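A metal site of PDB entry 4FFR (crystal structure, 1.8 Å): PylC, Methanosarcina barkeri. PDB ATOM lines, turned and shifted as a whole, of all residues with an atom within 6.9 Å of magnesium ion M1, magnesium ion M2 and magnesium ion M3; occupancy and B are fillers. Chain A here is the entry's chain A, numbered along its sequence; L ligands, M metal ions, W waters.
NZ of Lys 104 lies close to O5 of the ligand (2.4 Å).
The guanidinium group of Arg 243 sits close to an oxygen (O3) of the ligand, 2.8 Å away.
O1 of the ligand is in hydrogen-bond range of N of Ser 137, 2.9 Å away.
N of Ser 138 lies within hydrogen-bond range of O4 of the ligand, 2.9 Å away.
The backbone NH of Ile 238 is in hydrogen-bond range of the backbone carbonyl oxygen of Glu 227, at 2.9 Å.
The side-chain carboxylate (OE1) of Glu 239 lies close to the side-chain amino group (NZ) of Lys 104, at 3.5 Å.
The guanidinium group (NH2) of Arg 243 lies close to the side-chain carboxylate (OD2) of Asp 241 (3.4 Å).
The backbone carbonyl oxygen (O) of Asp 241 sits at hydrogen-bond distance from the backbone NH (N) of Asp 225 (3.0 Å).
OG of Ser 101 is in hydrogen-bond range of N of Ala 242, at 2.9 Å.
The side-chain amino group (NZ) of Lys 104 sits at hydrogen-bond distance from the backbone carbonyl oxygen (O) of Glu 135 (3.1 Å).
The backbone NH of Lys 104 lies within hydrogen-bond range of the backbone carbonyl oxygen of Pro 133 (2.8 Å).
Within 4 Å of magnesium ion M1: Ser 101, Glu 239, Ile 240 and Asp 241.
Merely in contact with magnesium ion M2: Lys 104 (3.97 Å).
The nearest printed residue that does not touch magnesium ion M3 is Asp 241 (4.4 Å).
Magnesium ion M1 is bound by OD1 of Asp 241 (1.9 Å), O of Ile 240 (2.2 Å), O of Ser 101 (2.2 Å) and water W2 (2.4 Å).
Magnesium ion M1 has four donor atoms within binding distance.
Slightly farther from magnesium ion M1 lies water W4 (2.6 Å).
Slightly farther from magnesium ion M1 lies the side-chain carboxylate (OE1) of Glu 239 (2.8 Å).
Magnesium ion M2 is bound by an oxygen (O5) of the ligand, an oxygen (O3) of the ligand, the side-chain carboxylate (OD2) of Asp 241, the side-chain carboxylate (OE2) of Glu 239, water W3, the side-chain carboxylate (OE1) of Glu 239 and an oxygen (O6) of the ligand.
Magnesium ion M3 is bound by O2 of the ligand.
Magnesium ion M3 is bound by OE2 of Glu 227, at 1.9 Å.
The side-chain carboxylate (OE2) of Glu 239 binds magnesium ion M3, 1.9 Å away.
An oxygen (O7) of the ligand binds magnesium ion M3 (1.9 Å).
Magnesium ion M3 is bound by an oxygen (O6) of the ligand (2.0 Å).
Magnesium ion M3 is bound by water W1, at 2.3 Å.
Magnesium ion M3 has six donor atoms within binding distance.
Water W2 lies within hydrogen-bond range of the side-chain amino group of Lys 104 (2.9 Å) and the backbone carbonyl oxygen of Arg 102 (2.9 Å).
Water W4 bridges the side-chain hydroxyl of Ser 107 (2.9 Å) and the backbone NH of Ile 240 (3.2 Å).
Water W1 bridges an oxygen (O12) of the ligand (2.7 Å) and the side-chain carboxylate (OE1) of Glu 227 (2.8 Å).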
ATOM      1  N   GLU A  72     -24.019  11.328  36.933  1.00  0.00           N
ATOM      2  CA  GLU A  72     -23.779  10.417  35.831  1.00  0.00           C
ATOM      3  C   GLU A  72     -22.386   9.807  35.898  1.00  0.00           C
ATOM      4  O   GLU A  72     -21.770   9.494  34.877  1.00  0.00           O
ATOM      5  CB  GLU A  72     -24.078  11.095  34.483  1.00  0.00           C
ATOM      6  CG  GLU A  72     -25.560  11.408  34.304  1.00  0.00           C
ATOM      7  CD  GLU A  72     -26.038  11.231  32.874  1.00  0.00           C
ATOM      8  OE1 GLU A  72     -26.028  10.084  32.376  1.00  0.00           O
ATOM      9  OE2 GLU A  72     -26.455  12.234  32.266  1.00  0.00           O
ATOM     10  N   ILE A 100     -29.106   1.256  29.091  1.00  0.00           N
ATOM     11  CA  ILE A 100     -29.438   1.491  27.694  1.00  0.00           C
ATOM     12  C   ILE A 100     -29.310   2.970  27.323  1.00  0.00           C
ATOM     13  O   ILE A 100     -28.675   3.306  26.324  1.00  0.00           O
ATOM     14  CB  ILE A 100     -30.856   0.983  27.348  1.00  0.00           C
ATOM     15  CG1 ILE A 100     -30.992  -0.508  27.684  1.00  0.00           C
ATOM     16  CG2 ILE A 100     -31.180   1.254  25.881  1.00  0.00           C
ATOM     17  CD1 ILE A 100     -32.407  -1.062  27.575  1.00  0.00           C
ATOM     18  N   SER A 101     -29.891   3.847  28.140  1.00  0.00           N
ATOM     19  CA  SER A 101     -30.014   5.272  27.796  1.00  0.00           C
ATOM     20  C   SER A 101     -28.685   6.021  27.762  1.00  0.00           C
ATOM     21  O   SER A 101     -28.503   6.968  26.995  1.00  0.00           O
ATOM     22  CB  SER A 101     -30.988   5.976  28.748  1.00  0.00           C
ATOM     23  OG  SER A 101     -30.416   6.177  30.034  1.00  0.00           O
ATOM     24  N   ARG A 102     -27.760   5.586  28.619  1.00  0.00           N
ATOM     25  CA  ARG A 102     -26.447   6.208  28.745  1.00  0.00           C
ATOM     26  C   ARG A 102     -25.617   6.010  27.478  1.00  0.00           C
ATOM     27  O   ARG A 102     -24.831   6.893  27.113  1.00  0.00           O
ATOM     28  CB  ARG A 102     -25.751   5.649  29.998  1.00  0.00           C
ATOM     29  CG  ARG A 102     -24.257   5.399  29.901  1.00  0.00           C
ATOM     30  CD  ARG A 102     -23.864   4.256  30.825  1.00  0.00           C
ATOM     31  NE  ARG A 102     -24.373   2.977  30.346  1.00  0.00           N
ATOM     32  CZ  ARG A 102     -23.640   2.049  29.744  1.00  0.00           C
ATOM     33  NH1 ARG A 102     -22.332   2.227  29.544  1.00  0.00           N
ATOM     34  NH2 ARG A 102     -24.197   0.920  29.335  1.00  0.00           N
ATOM     35  N   ASP A 103     -25.817   4.886  26.794  1.00  0.00           N
ATOM     36  CA  ASP A 103     -25.074   4.550  25.590  1.00  0.00           C
ATOM     37  C   ASP A 103     -25.919   4.868  24.357  1.00  0.00           C
ATOM     38  O   ASP A 103     -26.876   4.156  24.053  1.00  0.00           O
ATOM     39  CB  ASP A 103     -24.712   3.063  25.622  1.00  0.00           C
ATOM     40  CG  ASP A 103     -23.805   2.627  24.475  1.00  0.00           C
ATOM     41  OD1 ASP A 103     -23.976   3.099  23.334  1.00  0.00           O
ATOM     42  OD2 ASP A 103     -22.930   1.782  24.723  1.00  0.00           O
ATOM     43  N   LYS A 104     -25.560   5.935  23.650  1.00  0.00           N
ATOM     44  CA  LYS A 104     -26.354   6.404  22.511  1.00  0.00           C
ATOM     45  C   LYS A 104     -26.512   5.366  21.395  1.00  0.00           C
ATOM     46  O   LYS A 104     -27.551   5.349  20.731  1.00  0.00           O
ATOM     47  CB  LYS A 104     -25.824   7.729  21.980  1.00  0.00           C
ATOM     48  CG  LYS A 104     -26.014   8.863  22.974  1.00  0.00           C
ATOM     49  CD  LYS A 104     -25.672  10.220  22.396  1.00  0.00           C
ATOM     50  CE  LYS A 104     -26.169  11.320  23.307  1.00  0.00           C
ATOM     51  NZ  LYS A 104     -25.510  11.320  24.644  1.00  0.00           N
ATOM     52  N   SER A 107     -29.029   2.780  22.710  1.00  0.00           N
ATOM     53  CA  SER A 107     -30.304   3.481  22.627  1.00  0.00           C
ATOM     54  C   SER A 107     -30.857   3.463  21.204  1.00  0.00           C
ATOM     55  O   SER A 107     -32.034   3.210  20.999  1.00  0.00           O
ATOM     56  CB  SER A 107     -30.160   4.933  23.116  1.00  0.00           C
ATOM     57  OG  SER A 107     -30.016   4.976  24.521  1.00  0.00           O
ATOM     58  N   PRO A 133     -20.437   8.728  22.472  1.00  0.00           N
ATOM     59  CA  PRO A 133     -21.556   7.830  22.731  1.00  0.00           C
ATOM     60  C   PRO A 133     -22.159   7.927  24.138  1.00  0.00           C
ATOM     61  O   PRO A 133     -23.293   7.488  24.342  1.00  0.00           O
ATOM     62  CB  PRO A 133     -20.953   6.440  22.506  1.00  0.00           C
ATOM     63  CG  PRO A 133     -19.507   6.607  22.827  1.00  0.00           C
ATOM     64  CD  PRO A 133     -19.149   8.011  22.405  1.00  0.00           C
ATOM     65  N   GLU A 135     -21.665  10.873  26.654  1.00  0.00           N
ATOM     66  CA  GLU A 135     -21.618  12.158  27.349  1.00  0.00           C
ATOM     67  C   GLU A 135     -23.021  12.738  27.565  1.00  0.00           C
ATOM     68  O   GLU A 135     -24.027  12.128  27.192  1.00  0.00           O
ATOM     69  CB  GLU A 135     -20.737  13.160  26.587  1.00  0.00           C
ATOM     70  CG  GLU A 135     -19.239  12.871  26.662  1.00  0.00           C
ATOM     71  CD  GLU A 135     -18.608  13.228  28.002  1.00  0.00           C
ATOM     72  OE1 GLU A 135     -17.546  12.658  28.316  1.00  0.00           O
ATOM     73  OE2 GLU A 135     -19.169  14.076  28.738  1.00  0.00           O
ATOM     74  N   SER A 136     -23.087  13.912  28.202  1.00  0.00           N
ATOM     75  CA  SER A 136     -24.338  14.662  28.338  1.00  0.00           C
ATOM     76  C   SER A 136     -24.054  16.155  28.211  1.00  0.00           C
ATOM     77  O   SER A 136     -22.895  16.551  28.029  1.00  0.00           O
ATOM     78  CB  SER A 136     -25.030  14.344  29.660  1.00  0.00           C
ATOM     79  OG  SER A 136     -24.183  14.612  30.764  1.00  0.00           O
ATOM     80  N   SER A 137     -25.102  16.976  28.303  1.00  0.00           N
ATOM     81  CA  SER A 137     -24.997  18.442  28.209  1.00  0.00           C
ATOM     82  C   SER A 137     -24.351  18.927  26.899  1.00  0.00           C
ATOM     83  O   SER A 137     -23.815  20.032  26.829  1.00  0.00           O
ATOM     84  CB  SER A 137     -24.231  19.017  29.424  1.00  0.00           C
ATOM     85  OG  SER A 137     -24.815  18.603  30.648  1.00  0.00           O
ATOM     86  N   SER A 138     -24.420  18.067  25.871  1.00  0.00           N
ATOM     87  CA  SER A 138     -23.858  18.352  24.537  1.00  0.00           C
ATOM     88  C   SER A 138     -22.330  18.418  24.511  1.00  0.00           C
ATOM     89  O   SER A 138     -21.746  18.965  23.565  1.00  0.00           O
ATOM     90  CB  SER A 138     -24.456  19.629  23.941  1.00  0.00           C
ATOM     91  OG  SER A 138     -25.873  19.641  24.072  1.00  0.00           O
ATOM     92  N   VAL A 167     -35.785  21.036  18.780  1.00  0.00           N
ATOM     93  CA  VAL A 167     -35.423  19.972  19.698  1.00  0.00           C
ATOM     94  C   VAL A 167     -36.458  19.950  20.824  1.00  0.00           C
ATOM     95  O   VAL A 167     -36.641  20.947  21.546  1.00  0.00           O
ATOM     96  CB  VAL A 167     -33.998  20.159  20.250  1.00  0.00           C
ATOM     97  CG1 VAL A 167     -33.661  19.027  21.232  1.00  0.00           C
ATOM     98  CG2 VAL A 167     -32.991  20.191  19.112  1.00  0.00           C
ATOM     99  N   ASP A 225     -36.289  11.017  30.190  1.00  0.00           N
ATOM    100  CA  ASP A 225     -36.698  12.001  29.212  1.00  0.00           C
ATOM    101  C   ASP A 225     -36.398  11.477  27.825  1.00  0.00           C
ATOM    102  O   ASP A 225     -35.468  10.685  27.617  1.00  0.00           O
ATOM    103  CB  ASP A 225     -36.083  13.389  29.479  1.00  0.00           C
ATOM    104  CG  ASP A 225     -34.723  13.555  28.846  1.00  0.00           C
ATOM    105  OD1 ASP A 225     -34.578  14.477  28.016  1.00  0.00           O
ATOM    106  OD2 ASP A 225     -33.817  12.765  29.170  1.00  0.00           O
ATOM    107  N   GLU A 227     -35.829  12.794  23.870  1.00  0.00           N
ATOM    108  CA  GLU A 227     -35.540  13.976  23.059  1.00  0.00           C
ATOM    109  C   GLU A 227     -35.695  13.636  21.590  1.00  0.00           C
ATOM    110  O   GLU A 227     -35.160  12.625  21.119  1.00  0.00           O
ATOM    111  CB  GLU A 227     -34.141  14.514  23.348  1.00  0.00           C
ATOM    112  CG  GLU A 227     -33.986  15.076  24.749  1.00  0.00           C
ATOM    113  CD  GLU A 227     -32.667  15.803  24.952  1.00  0.00           C
ATOM    114  OE1 GLU A 227     -32.721  17.024  25.248  1.00  0.00           O
ATOM    115  OE2 GLU A 227     -31.599  15.182  24.803  1.00  0.00           O
ATOM    116  N   ILE A 238     -33.602  11.410  19.029  1.00  0.00           N
ATOM    117  CA  ILE A 238     -32.139  11.475  19.060  1.00  0.00           C
ATOM    118  C   ILE A 238     -31.552  10.752  20.260  1.00  0.00           C
ATOM    119  O   ILE A 238     -30.515  10.092  20.134  1.00  0.00           O
ATOM    120  CB  ILE A 238     -31.588  12.927  18.934  1.00  0.00           C
ATOM    121  CG1 ILE A 238     -32.091  13.826  20.075  1.00  0.00           C
ATOM    122  CG2 ILE A 238     -31.915  13.497  17.551  1.00  0.00           C
ATOM    123  CD1 ILE A 238     -31.447  15.205  20.128  1.00  0.00           C
ATOM    124  N   GLU A 239     -32.204  10.842  21.406  1.00  0.00           N
ATOM    125  CA  GLU A 239     -31.742  10.142  22.599  1.00  0.00           C
ATOM    126  C   GLU A 239     -32.806   9.988  23.672  1.00  0.00           C
ATOM    127  O   GLU A 239     -33.865  10.614  23.641  1.00  0.00           O
ATOM    128  CB  GLU A 239     -30.492  10.826  23.193  1.00  0.00           C
ATOM    129  CG  GLU A 239     -30.759  12.184  23.830  1.00  0.00           C
ATOM    130  CD  GLU A 239     -29.745  12.519  24.912  1.00  0.00           C
ATOM    131  OE1 GLU A 239     -28.951  11.633  25.291  1.00  0.00           O
ATOM    132  OE2 GLU A 239     -29.753  13.682  25.404  1.00  0.00           O
ATOM    133  N   ILE A 240     -32.503   9.108  24.615  1.00  0.00           N
ATOM    134  CA  ILE A 240     -33.239   8.997  25.857  1.00  0.00           C
ATOM    135  C   ILE A 240     -32.210   9.119  26.978  1.00  0.00           C
ATOM    136  O   ILE A 240     -31.023   8.818  26.786  1.00  0.00           O
ATOM    137  CB  ILE A 240     -34.022   7.675  25.960  1.00  0.00           C
ATOM    138  CG1 ILE A 240     -33.117   6.476  25.651  1.00  0.00           C
ATOM    139  CG2 ILE A 240     -35.227   7.702  25.007  1.00  0.00           C
ATOM    140  CD1 ILE A 240     -33.719   5.116  25.945  1.00  0.00           C
ATOM    141  N   ASP A 241     -32.639   9.612  28.128  1.00  0.00           N
ATOM    142  CA  ASP A 241     -31.756   9.668  29.299  1.00  0.00           C
ATOM    143  C   ASP A 241     -32.615   9.275  30.516  1.00  0.00           C
ATOM    144  O   ASP A 241     -33.536  10.000  30.920  1.00  0.00           O
ATOM    145  CB  ASP A 241     -31.019  11.054  29.404  1.00  0.00           C
ATOM    146  CG  ASP A 241     -29.773  11.196  28.419  1.00  0.00           C
ATOM    147  OD1 ASP A 241     -29.134  10.149  28.110  1.00  0.00           O
ATOM    148  OD2 ASP A 241     -29.409  12.351  27.967  1.00  0.00           O
ATOM    149  N   ALA A 242     -32.358   8.074  31.035  1.00  0.00           N
ATOM    150  CA  ALA A 242     -33.128   7.520  32.159  1.00  0.00           C
ATOM    151  C   ALA A 242     -32.486   7.921  33.487  1.00  0.00           C
ATOM    152  O   ALA A 242     -31.845   7.117  34.178  1.00  0.00           O
ATOM    153  CB  ALA A 242     -33.256   6.003  32.050  1.00  0.00           C
ATOM    154  N   ARG A 243     -32.643   9.201  33.812  1.00  0.00           N
ATOM    155  CA  ARG A 243     -32.202   9.795  35.077  1.00  0.00           C
ATOM    156  C   ARG A 243     -32.966  11.097  35.231  1.00  0.00           C
ATOM    157  O   ARG A 243     -33.635  11.541  34.290  1.00  0.00           O
ATOM    158  CB  ARG A 243     -30.673  10.012  35.116  1.00  0.00           C
ATOM    159  CG  ARG A 243     -30.028  10.472  33.806  1.00  0.00           C
ATOM    160  CD  ARG A 243     -30.342  11.913  33.455  1.00  0.00           C
ATOM    161  NE  ARG A 243     -29.339  12.479  32.552  1.00  0.00           N
ATOM    162  CZ  ARG A 243     -29.576  13.384  31.604  1.00  0.00           C
ATOM    163  NH1 ARG A 243     -30.809  13.829  31.392  1.00  0.00           N
ATOM    164  NH2 ARG A 243     -28.581  13.835  30.862  1.00  0.00           N
HETATM  165  P1  LIG L   1     -28.546  15.715  27.144  1.00  0.00           P
HETATM  166  O1  LIG L   1     -27.930  17.016  27.583  1.00  0.00           O
HETATM  167  O2  LIG L   1     -30.028  15.902  26.884  1.00  0.00           O
HETATM  168  O3  LIG L   1     -28.140  14.689  28.179  1.00  0.00           O
HETATM  169  P2  LIG L   1     -26.666  14.573  25.271  1.00  0.00           P
HETATM  170  O4  LIG L   1     -25.437  15.446  25.399  1.00  0.00           O
HETATM  171  O5  LIG L   1     -26.592  13.170  25.776  1.00  0.00           O
HETATM  172  O6  LIG L   1     -27.892  15.509  25.680  1.00  0.00           O
HETATM  173  P3  LIG L   1     -27.814  14.801  22.541  1.00  0.00           P
HETATM  174  O7  LIG L   1     -29.065  15.250  23.270  1.00  0.00           O
HETATM  175  O8  LIG L   1     -27.862  13.604  21.621  1.00  0.00           O
HETATM  176  O9  LIG L   1     -26.637  14.554  23.631  1.00  0.00           O
HETATM  177  O10 LIG L   1     -27.267  16.025  21.651  1.00  0.00           O
HETATM  178  C1  LIG L   1     -27.139  17.343  22.191  1.00  0.00           C
HETATM  179  C2  LIG L   1     -27.694  18.374  21.214  1.00  0.00           C
HETATM  180  O11 LIG L   1     -27.078  18.259  19.934  1.00  0.00           O
HETATM  181  C3  LIG L   1     -29.191  18.198  20.962  1.00  0.00           C
HETATM  182  O12 LIG L   1     -30.006  18.855  21.932  1.00  0.00           O
HETATM  183  C4  LIG L   1     -29.360  18.790  19.585  1.00  0.00           C
HETATM  184  O13 LIG L   1     -29.422  20.213  19.652  1.00  0.00           O
HETATM  185  C5  LIG L   1     -28.054  18.432  18.897  1.00  0.00           C
HETATM  186  N1  LIG L   1     -28.120  17.186  18.097  1.00  0.00           N
HETATM  187  C6  LIG L   1     -27.859  15.932  18.535  1.00  0.00           C
HETATM  188  N2  LIG L   1     -27.960  15.016  17.536  1.00  0.00           N
HETATM  189  C7  LIG L   1     -28.309  15.700  16.424  1.00  0.00           C
HETATM  190  C8  LIG L   1     -28.585  15.362  15.011  1.00  0.00           C
HETATM  191  N3  LIG L   1     -28.520  14.085  14.570  1.00  0.00           N
HETATM  192  N4  LIG L   1     -28.901  16.377  14.173  1.00  0.00           N
HETATM  193  C9  LIG L   1     -28.958  17.667  14.580  1.00  0.00           C
HETATM  194  N5  LIG L   1     -28.722  18.040  15.842  1.00  0.00           N
HETATM  195  C10 LIG L   1     -28.393  17.126  16.796  1.00  0.00           C
HETATM  196 MG    MG M   1     -28.866   9.088  26.511  1.00  0.00          MG
HETATM  197 MG    MG M   2     -28.116  13.347  26.854  1.00  0.00          MG
HETATM  198 MG    MG M   3     -29.742  15.561  25.035  1.00  0.00          MG
HETATM  199  O   HOH W   1     -30.120  17.777  24.384  1.00  0.00           O
HETATM  200  O   HOH W   2     -26.468   9.240  26.415  1.00  0.00           O
HETATM  201  O   HOH W   3     -26.676  11.753  28.012  1.00  0.00           O
HETATM  202  O   HOH W   4     -29.547   7.857  24.282  1.00  0.00           O
